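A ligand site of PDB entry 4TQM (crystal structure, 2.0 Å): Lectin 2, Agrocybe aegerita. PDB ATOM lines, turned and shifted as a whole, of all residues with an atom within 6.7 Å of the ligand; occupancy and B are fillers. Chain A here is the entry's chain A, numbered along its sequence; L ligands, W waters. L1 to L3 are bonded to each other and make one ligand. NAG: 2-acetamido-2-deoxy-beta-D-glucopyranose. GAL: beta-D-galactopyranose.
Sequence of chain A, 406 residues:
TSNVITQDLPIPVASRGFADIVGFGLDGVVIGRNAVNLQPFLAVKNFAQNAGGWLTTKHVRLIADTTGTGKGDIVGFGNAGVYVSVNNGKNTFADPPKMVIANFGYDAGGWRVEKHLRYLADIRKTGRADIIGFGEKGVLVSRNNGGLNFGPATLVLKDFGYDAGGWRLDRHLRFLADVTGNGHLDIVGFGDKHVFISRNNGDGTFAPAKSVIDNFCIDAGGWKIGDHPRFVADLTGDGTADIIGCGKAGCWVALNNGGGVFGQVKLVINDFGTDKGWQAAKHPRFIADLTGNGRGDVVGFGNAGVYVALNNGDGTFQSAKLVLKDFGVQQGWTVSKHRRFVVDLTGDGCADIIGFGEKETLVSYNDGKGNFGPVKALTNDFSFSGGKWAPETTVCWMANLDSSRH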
ATOM      1  N   LYS A  45      10.664  19.588  -8.203  1.00  0.00           N
ATOM      2  CA  LYS A  45      10.982  18.731  -9.345  1.00  0.00           C
ATOM      3  C   LYS A  45      12.039  19.398 -10.221  1.00  0.00           C
ATOM      4  O   LYS A  45      11.775  19.804 -11.356  1.00  0.00           O
ATOM      5  CB  LYS A  45       9.720  18.393 -10.139  1.00  0.00           C
ATOM      6  CG  LYS A  45       8.763  17.492  -9.388  1.00  0.00           C
ATOM      7  CD  LYS A  45       7.532  17.135 -10.207  1.00  0.00           C
ATOM      8  CE  LYS A  45       6.677  16.102  -9.493  1.00  0.00           C
ATOM      9  NZ  LYS A  45       5.442  15.749 -10.251  1.00  0.00           N
ATOM     10  N   ASN A  46      13.248  19.512  -9.666  1.00  0.00           N
ATOM     11  CA  ASN A  46      14.352  20.193 -10.327  1.00  0.00           C
ATOM     12  C   ASN A  46      15.623  19.890  -9.539  1.00  0.00           C
ATOM     13  O   ASN A  46      15.597  19.098  -8.596  1.00  0.00           O
ATOM     14  CB  ASN A  46      14.085  21.702 -10.372  1.00  0.00           C
ATOM     15  CG  ASN A  46      14.791  22.389 -11.536  1.00  0.00           C
ATOM     16  OD1 ASN A  46      15.952  22.086 -11.833  1.00  0.00           O
ATOM     17  ND2 ASN A  46      14.094  23.305 -12.193  1.00  0.00           N
ATOM     18  N   PHE A  47      16.736  20.530  -9.923  1.00  0.00           N
ATOM     19  CA  PHE A  47      18.033  20.304  -9.285  1.00  0.00           C
ATOM     20  C   PHE A  47      18.415  18.828  -9.273  1.00  0.00           C
ATOM     21  O   PHE A  47      19.069  18.350  -8.340  1.00  0.00           O
ATOM     22  CB  PHE A  47      18.043  20.857  -7.851  1.00  0.00           C
ATOM     23  CG  PHE A  47      17.671  22.305  -7.753  1.00  0.00           C
ATOM     24  CD1 PHE A  47      18.635  23.291  -7.905  1.00  0.00           C
ATOM     25  CD2 PHE A  47      16.368  22.695  -7.494  1.00  0.00           C
ATOM     26  CE1 PHE A  47      18.305  24.631  -7.811  1.00  0.00           C
ATOM     27  CE2 PHE A  47      16.027  24.039  -7.391  1.00  0.00           C
ATOM     28  CZ  PHE A  47      17.000  25.002  -7.548  1.00  0.00           C
ATOM     29  N   ALA A  48      18.013  18.094 -10.314  1.00  0.00           N
ATOM     30  CA  ALA A  48      18.136  16.641 -10.309  1.00  0.00           C
ATOM     31  C   ALA A  48      18.698  16.064 -11.608  1.00  0.00           C
ATOM     32  O   ALA A  48      18.597  16.677 -12.670  1.00  0.00           O
ATOM     33  CB  ALA A  48      16.799  16.013 -10.011  1.00  0.00           C
ATOM     34  N   ALA A  51      15.745  15.717 -13.743  1.00  0.00           N
ATOM     35  CA  ALA A  51      14.838  16.854 -13.701  1.00  0.00           C
ATOM     36  C   ALA A  51      15.639  18.149 -13.738  1.00  0.00           C
ATOM     37  O   ALA A  51      16.006  18.691 -12.695  1.00  0.00           O
ATOM     38  CB  ALA A  51      13.967  16.799 -12.455  1.00  0.00           C
ATOM     39  N   GLY A  52      15.919  18.642 -14.939  1.00  0.00           N
ATOM     40  CA  GLY A  52      16.711  19.848 -15.099  1.00  0.00           C
ATOM     41  C   GLY A  52      18.090  19.550 -15.643  1.00  0.00           C
ATOM     42  O   GLY A  52      18.850  20.461 -15.984  1.00  0.00           O
ATOM     43  N   GLY A  53      18.424  18.265 -15.719  1.00  0.00           N
ATOM     44  CA  GLY A  53      19.702  17.832 -16.267  1.00  0.00           C
ATOM     45  C   GLY A  53      20.889  18.174 -15.397  1.00  0.00           C
ATOM     46  O   GLY A  53      21.940  18.588 -15.895  1.00  0.00           O
ATOM     47  N   TRP A  54      20.739  18.014 -14.082  1.00  0.00           N
ATOM     48  CA  TRP A  54      21.821  18.347 -13.162  1.00  0.00           C
ATOM     49  C   TRP A  54      22.824  17.205 -13.004  1.00  0.00           C
ATOM     50  O   TRP A  54      22.447  16.028 -12.995  1.00  0.00           O
ATOM     51  CB  TRP A  54      21.243  18.772 -11.809  1.00  0.00           C
ATOM     52  CG  TRP A  54      20.560  20.103 -11.863  1.00  0.00           C
ATOM     53  CD1 TRP A  54      19.353  20.389 -12.428  1.00  0.00           C
ATOM     54  CD2 TRP A  54      21.057  21.342 -11.325  1.00  0.00           C
ATOM     55  NE1 TRP A  54      19.070  21.725 -12.289  1.00  0.00           N
ATOM     56  CE2 TRP A  54      20.089  22.328 -11.611  1.00  0.00           C
ATOM     57  CE3 TRP A  54      22.217  21.707 -10.636  1.00  0.00           C
ATOM     58  CZ2 TRP A  54      20.253  23.664 -11.235  1.00  0.00           C
ATOM     59  CZ3 TRP A  54      22.380  23.034 -10.258  1.00  0.00           C
ATOM     60  CH2 TRP A  54      21.401  23.987 -10.557  1.00  0.00           C
ATOM     61  N   LEU A  55      24.102  17.563 -12.883  1.00  0.00           N
ATOM     62  CA  LEU A  55      25.184  16.580 -12.809  1.00  0.00           C
ATOM     63  C   LEU A  55      26.188  16.957 -11.728  1.00  0.00           C
ATOM     64  O   LEU A  55      26.597  18.117 -11.619  1.00  0.00           O
ATOM     65  CB  LEU A  55      25.920  16.502 -14.153  1.00  0.00           C
ATOM     66  CG  LEU A  55      25.175  15.986 -15.374  1.00  0.00           C
ATOM     67  CD1 LEU A  55      25.949  16.327 -16.629  1.00  0.00           C
ATOM     68  CD2 LEU A  55      24.966  14.485 -15.271  1.00  0.00           C
ATOM     69  N   LYS A  58      29.308  18.671 -13.017  1.00  0.00           N
ATOM     70  CA  LYS A  58      29.204  19.993 -13.638  1.00  0.00           C
ATOM     71  C   LYS A  58      28.595  21.043 -12.718  1.00  0.00           C
ATOM     72  O   LYS A  58      28.767  22.244 -12.938  1.00  0.00           O
ATOM     73  CB  LYS A  58      28.357  19.919 -14.904  1.00  0.00           C
ATOM     74  CG  LYS A  58      29.066  19.358 -16.117  1.00  0.00           C
ATOM     75  CD  LYS A  58      28.305  19.728 -17.390  1.00  0.00           C
ATOM     76  CE  LYS A  58      29.053  19.260 -18.634  1.00  0.00           C
ATOM     77  NZ  LYS A  58      29.236  17.790 -18.633  1.00  0.00           N
ATOM     78  N   HIS A  59      27.888  20.603 -11.694  1.00  0.00           N
ATOM     79  CA  HIS A  59      27.057  21.516 -10.928  1.00  0.00           C
ATOM     80  C   HIS A  59      27.218  21.379  -9.429  1.00  0.00           C
ATOM     81  O   HIS A  59      27.664  20.338  -8.929  1.00  0.00           O
ATOM     82  CB  HIS A  59      25.591  21.340 -11.326  1.00  0.00           C
ATOM     83  CG  HIS A  59      25.379  21.364 -12.801  1.00  0.00           C
ATOM     84  ND1 HIS A  59      24.875  20.285 -13.499  1.00  0.00           N
ATOM     85  CD2 HIS A  59      25.637  22.314 -13.719  1.00  0.00           C
ATOM     86  CE1 HIS A  59      24.813  20.585 -14.785  1.00  0.00           C
ATOM     87  NE2 HIS A  59      25.275  21.812 -14.945  1.00  0.00           N
ATOM     88  N   GLY A  76      21.299  26.089  -6.302  1.00  0.00           N
ATOM     89  CA  GLY A  76      21.975  25.291  -7.308  1.00  0.00           C
ATOM     90  C   GLY A  76      22.790  26.094  -8.319  1.00  0.00           C
ATOM     91  O   GLY A  76      22.242  26.889  -9.085  1.00  0.00           O
ATOM     92  N   PHE A  77      24.099  25.881  -8.300  1.00  0.00           N
ATOM     93  CA  PHE A  77      25.002  26.412  -9.295  1.00  0.00           C
ATOM     94  C   PHE A  77      24.940  25.509 -10.527  1.00  0.00           C
ATOM     95  O   PHE A  77      25.591  24.448 -10.569  1.00  0.00           O
ATOM     96  CB  PHE A  77      26.438  26.447  -8.763  1.00  0.00           C
ATOM     97  CG  PHE A  77      26.609  27.325  -7.551  1.00  0.00           C
ATOM     98  CD1 PHE A  77      27.036  28.644  -7.683  1.00  0.00           C
ATOM     99  CD2 PHE A  77      26.364  26.837  -6.267  1.00  0.00           C
ATOM    100  CE1 PHE A  77      27.210  29.456  -6.579  1.00  0.00           C
ATOM    101  CE2 PHE A  77      26.538  27.651  -5.153  1.00  0.00           C
ATOM    102  CZ  PHE A  77      26.955  28.955  -5.313  1.00  0.00           C
ATOM    103  N   GLY A  78      24.134  25.929 -11.506  1.00  0.00           N
ATOM    104  CA  GLY A  78      23.879  25.155 -12.705  1.00  0.00           C
ATOM    105  C   GLY A  78      24.598  25.716 -13.922  1.00  0.00           C
ATOM    106  O   GLY A  78      25.699  26.244 -13.807  1.00  0.00           O
ATOM    107  N   ASN A  79      23.973  25.610 -15.098  1.00  0.00           N
ATOM    108  CA  ASN A  79      24.640  26.007 -16.331  1.00  0.00           C
ATOM    109  C   ASN A  79      24.599  27.501 -16.618  1.00  0.00           C
ATOM    110  O   ASN A  79      25.644  28.146 -16.739  1.00  0.00           O
ATOM    111  CB  ASN A  79      24.091  25.212 -17.518  1.00  0.00           C
ATOM    112  CG  ASN A  79      24.526  23.764 -17.500  1.00  0.00           C
ATOM    113  OD1 ASN A  79      25.625  23.435 -17.033  1.00  0.00           O
ATOM    114  ND2 ASN A  79      23.673  22.874 -18.012  1.00  0.00           N
ATOM    115  N   ALA A  80      23.405  28.066 -16.724  1.00  0.00           N
ATOM    116  CA  ALA A  80      23.262  29.465 -17.107  1.00  0.00           C
ATOM    117  C   ALA A  80      23.382  30.423 -15.926  1.00  0.00           C
ATOM    118  O   ALA A  80      23.382  31.648 -16.108  1.00  0.00           O
ATOM    119  CB  ALA A  80      21.940  29.683 -17.837  1.00  0.00           C
ATOM    120  N   GLY A  81      23.508  29.873 -14.713  1.00  0.00           N
ATOM    121  CA  GLY A  81      23.647  30.696 -13.531  1.00  0.00           C
ATOM    122  C   GLY A  81      23.244  29.985 -12.254  1.00  0.00           C
ATOM    123  O   GLY A  81      23.231  28.754 -12.195  1.00  0.00           O
ATOM    124  N   TYR A  83      20.418  29.071  -9.411  1.00  0.00           N
ATOM    125  CA  TYR A  83      18.985  28.927  -9.199  1.00  0.00           C
ATOM    126  C   TYR A  83      18.675  28.788  -7.722  1.00  0.00           C
ATOM    127  O   TYR A  83      19.409  28.145  -6.982  1.00  0.00           O
ATOM    128  CB  TYR A  83      18.462  27.694  -9.944  1.00  0.00           C
ATOM    129  CG  TYR A  83      18.540  27.810 -11.437  1.00  0.00           C
ATOM    130  CD1 TYR A  83      17.421  28.149 -12.185  1.00  0.00           C
ATOM    131  CD2 TYR A  83      19.732  27.572 -12.117  1.00  0.00           C
ATOM    132  CE1 TYR A  83      17.480  28.252 -13.563  1.00  0.00           C
ATOM    133  CE2 TYR A  83      19.812  27.685 -13.486  1.00  0.00           C
ATOM    134  CZ  TYR A  83      18.680  28.022 -14.203  1.00  0.00           C
ATOM    135  OH  TYR A  83      18.749  28.124 -15.580  1.00  0.00           O
ATOM    136  N   PRO A  96       8.719  26.389 -10.009  1.00  0.00           N
ATOM    137  CA  PRO A  96      10.152  26.323 -10.327  1.00  0.00           C
ATOM    138  C   PRO A  96      11.003  27.311  -9.520  1.00  0.00           C
ATOM    139  O   PRO A  96      10.456  28.240  -8.929  1.00  0.00           O
ATOM    140  CB  PRO A  96      10.181  26.715 -11.804  1.00  0.00           C
ATOM    141  CG  PRO A  96       9.039  27.646 -11.951  1.00  0.00           C
ATOM    142  CD  PRO A  96       7.961  27.099 -11.053  1.00  0.00           C
ATOM    143  N   PRO A  97      12.333  27.106  -9.501  1.00  0.00           N
ATOM    144  CA  PRO A  97      13.232  28.062  -8.859  1.00  0.00           C
ATOM    145  C   PRO A  97      13.389  29.318  -9.698  1.00  0.00           C
ATOM    146  O   PRO A  97      12.916  29.373 -10.833  1.00  0.00           O
ATOM    147  CB  PRO A  97      14.566  27.303  -8.825  1.00  0.00           C
ATOM    148  CG  PRO A  97      14.486  26.358  -9.976  1.00  0.00           C
ATOM    149  CD  PRO A  97      13.043  25.916  -9.993  1.00  0.00           C
ATOM    150  N   MET A  99      16.317  32.035 -11.281  1.00  0.00           N
ATOM    151  CA  MET A  99      17.740  32.292 -11.499  1.00  0.00           C
ATOM    152  C   MET A  99      18.089  33.677 -10.972  1.00  0.00           C
ATOM    153  O   MET A  99      17.632  34.681 -11.504  1.00  0.00           O
ATOM    154  CB  MET A  99      18.132  32.207 -12.972  1.00  0.00           C
ATOM    155  CG  MET A  99      19.581  32.669 -13.185  1.00  0.00           C
ATOM    156  SD  MET A  99      20.110  32.712 -14.897  1.00  0.00           S
ATOM    157  CE  MET A  99      19.957  30.988 -15.295  1.00  0.00           C
ATOM    158  N   ASP A 107      28.248  27.084 -17.726  1.00  0.00           N
ATOM    159  CA  ASP A 107      28.242  27.890 -18.941  1.00  0.00           C
ATOM    160  C   ASP A 107      28.511  29.356 -18.632  1.00  0.00           C
ATOM    161  O   ASP A 107      29.485  29.936 -19.111  1.00  0.00           O
ATOM    162  CB  ASP A 107      26.922  27.731 -19.696  1.00  0.00           C
ATOM    163  CG  ASP A 107      26.773  26.364 -20.331  1.00  0.00           C
ATOM    164  OD1 ASP A 107      27.810  25.700 -20.549  1.00  0.00           O
ATOM    165  OD2 ASP A 107      25.624  25.965 -20.622  1.00  0.00           O
HETATM  166  C1  NAG L   1      25.160  23.646 -24.349  1.00  0.00           C
HETATM  167  C2  NAG L   1      23.935  24.467 -24.742  1.00  0.00           C
HETATM  168  C3  NAG L   1      23.220  24.962 -23.503  1.00  0.00           C
HETATM  169  C4  NAG L   1      22.934  23.816 -22.552  1.00  0.00           C
HETATM  170  C5  NAG L   1      24.176  22.972 -22.297  1.00  0.00           C
HETATM  171  C6  NAG L   1      23.831  21.738 -21.481  1.00  0.00           C
HETATM  172  C7  NAG L   1      23.654  25.850 -26.700  1.00  0.00           C
HETATM  173  C8  NAG L   1      24.054  27.097 -27.434  1.00  0.00           C
HETATM  174  N2  NAG L   1      24.313  25.589 -25.581  1.00  0.00           N
HETATM  175  O1  NAG L   1      25.800  23.146 -25.508  1.00  0.00           O
HETATM  176  O3  NAG L   1      22.008  25.594 -23.862  1.00  0.00           O
HETATM  177  O4  NAG L   1      22.453  24.346 -21.331  1.00  0.00           O
HETATM  178  O5  NAG L   1      24.787  22.575 -23.511  1.00  0.00           O
HETATM  179  O6  NAG L   1      22.960  20.921 -22.227  1.00  0.00           O
HETATM  180  O7  NAG L   1      22.750  25.138 -27.133  1.00  0.00           O
HETATM  181  C1  GAL L   2      21.037  24.229 -21.041  1.00  0.00           C
HETATM  182  C2  GAL L   2      20.955  24.324 -19.526  1.00  0.00           C
HETATM  183  C3  GAL L   2      19.540  24.698 -19.114  1.00  0.00           C
HETATM  184  C4  GAL L   2      19.087  25.954 -19.849  1.00  0.00           C
HETATM  185  C5  GAL L   2      19.336  25.813 -21.357  1.00  0.00           C
HETATM  186  C6  GAL L   2      19.007  27.111 -22.085  1.00  0.00           C
HETATM  187  O2  GAL L   2      21.329  23.094 -18.935  1.00  0.00           O
HETATM  188  O3  GAL L   2      19.506  24.916 -17.718  1.00  0.00           O
HETATM  189  O4  GAL L   2      19.767  27.077 -19.338  1.00  0.00           O
HETATM  190  O5  GAL L   2      20.692  25.487 -21.587  1.00  0.00           O
HETATM  191  O6  GAL L   2      19.359  26.993 -23.449  1.00  0.00           O
HETATM  192  C1  NAG L   3      18.323  24.359 -17.089  1.00  0.00           C
HETATM  193  C2  NAG L   3      18.517  24.127 -15.587  1.00  0.00           C
HETATM  194  C3  NAG L   3      17.204  23.735 -14.921  1.00  0.00           C
HETATM  195  C4  NAG L   3      16.123  24.748 -15.269  1.00  0.00           C
HETATM  196  C5  NAG L   3      16.010  24.846 -16.788  1.00  0.00           C
HETATM  197  C6  NAG L   3      14.943  25.852 -17.206  1.00  0.00           C
HETATM  198  C7  NAG L   3      20.795  23.459 -15.119  1.00  0.00           C
HETATM  199  C8  NAG L   3      21.764  22.356 -14.847  1.00  0.00           C
HETATM  200  N2  NAG L   3      19.536  23.111 -15.365  1.00  0.00           N
HETATM  201  O3  NAG L   3      17.378  23.664 -13.530  1.00  0.00           O
HETATM  202  O4  NAG L   3      14.888  24.355 -14.712  1.00  0.00           O
HETATM  203  O5  NAG L   3      17.256  25.262 -17.329  1.00  0.00           O
HETATM  204  O6  NAG L   3      15.340  27.135 -16.786  1.00  0.00           O
HETATM  205  O7  NAG L   3      21.162  24.637 -15.128  1.00  0.00           O
HETATM  206  O   HOH W   1      19.011  21.225 -18.394  1.00  0.00           O
HETATM  207  O   HOH W   2      18.084  29.304 -19.134  1.00  0.00           O
HETATM  208  O   HOH W   3      20.965  26.766 -16.537  1.00  0.00           O
HETATM  209  O   HOH W   4      13.552  22.075 -15.695  1.00  0.00           O
HETATM  210  O   HOH W   5      23.497  27.432 -20.416  1.00  0.00           O
HETATM  211  O   HOH W   6      18.895  29.214 -24.974  1.00  0.00           O
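O7 of NAG L3 is in hydrogen-bond range of N of Asn 79. The side-chain amide nitrogen of Asn 79 sits at hydrogen-bond distance from an oxygen (O2) of GAL L2 (2.5 Å). The side-chain amide oxygen (OD1) of Asn 46 sits at hydrogen-bond distance from an oxygen (O3) of NAG L3, at 2.7 Å. The backbone carbonyl oxygen of Gly 52 is in hydrogen-bond range of a nitrogen (N2) of NAG L3 (2.8 Å). NE1 of Trp 54 sits at hydrogen-bond distance from O3 of NAG L3 (2.9 Å).
OD1 of Asn 79 sits at hydrogen-bond distance from NE2 of His 59 (2.7 Å). The backbone carbonyl oxygen of Asn 79 is in hydrogen-bond range of the backbone NH of Asp 107. OD1 of Asn 46 lies within hydrogen-bond range of NE1 of Trp 54 (3.2 Å). The backbone carbonyl oxygen (O) of Ala 48 lies within hydrogen-bond range of the backbone NH (N) of Trp 54 (2.9 Å). ND1 of His 59 is in hydrogen-bond range of N of Leu 55. The backbone carbonyl oxygen of Gly 76 lies within hydrogen-bond range of the backbone NH of Tyr 83. The backbone NH (N) of Gly 53 is in hydrogen-bond range of the backbone carbonyl oxygen (O) of Ala 48 (3.4 Å).
O of Gly 53 touches C8 of NAG L3, 3.9 Å away. CE1 of His 59 touches C8 of NAG L3, at 3.5 Å. CA of Gly 78 touches O7 of NAG L3, at 3.7 Å. CB of Ala 80 touches O4 of GAL L2, at 3.7 Å. OH of Tyr 83 touches O5 of NAG L3 (3.7 Å). OD2 of Asp 107 touches O4 of NAG L1, 3.6 Å away. Hydrophobic or aromatic side chains that line the ligand: Trp 54, His 59, Ala 80 and Tyr 83. Ten residues have an atom within 4 Å of the ligand: Asn 46, Gly 52, Gly 53, Trp 54, His 59, Gly 78, Asn 79, Ala 80, Tyr 83 and Asp 107. The nearest printed residue that does not touch the ligand is Phe 47 (4.8 Å).
Water W3 lies within hydrogen-bond range of O7 of NAG L3 (2.6 Å), OH of Tyr 83 (2.8 Å) and N of Ala 80 (2.8 Å). Water W1 lies within hydrogen-bond range of the backbone carbonyl oxygen of Gly 52 (2.5 Å) and an oxygen (O2) of GAL L2 (3.0 Å). Water W5 bridges the side-chain carboxylate of Asp 107 (2.6 Å) and an oxygen (O4) of NAG L1 (3.4 Å).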
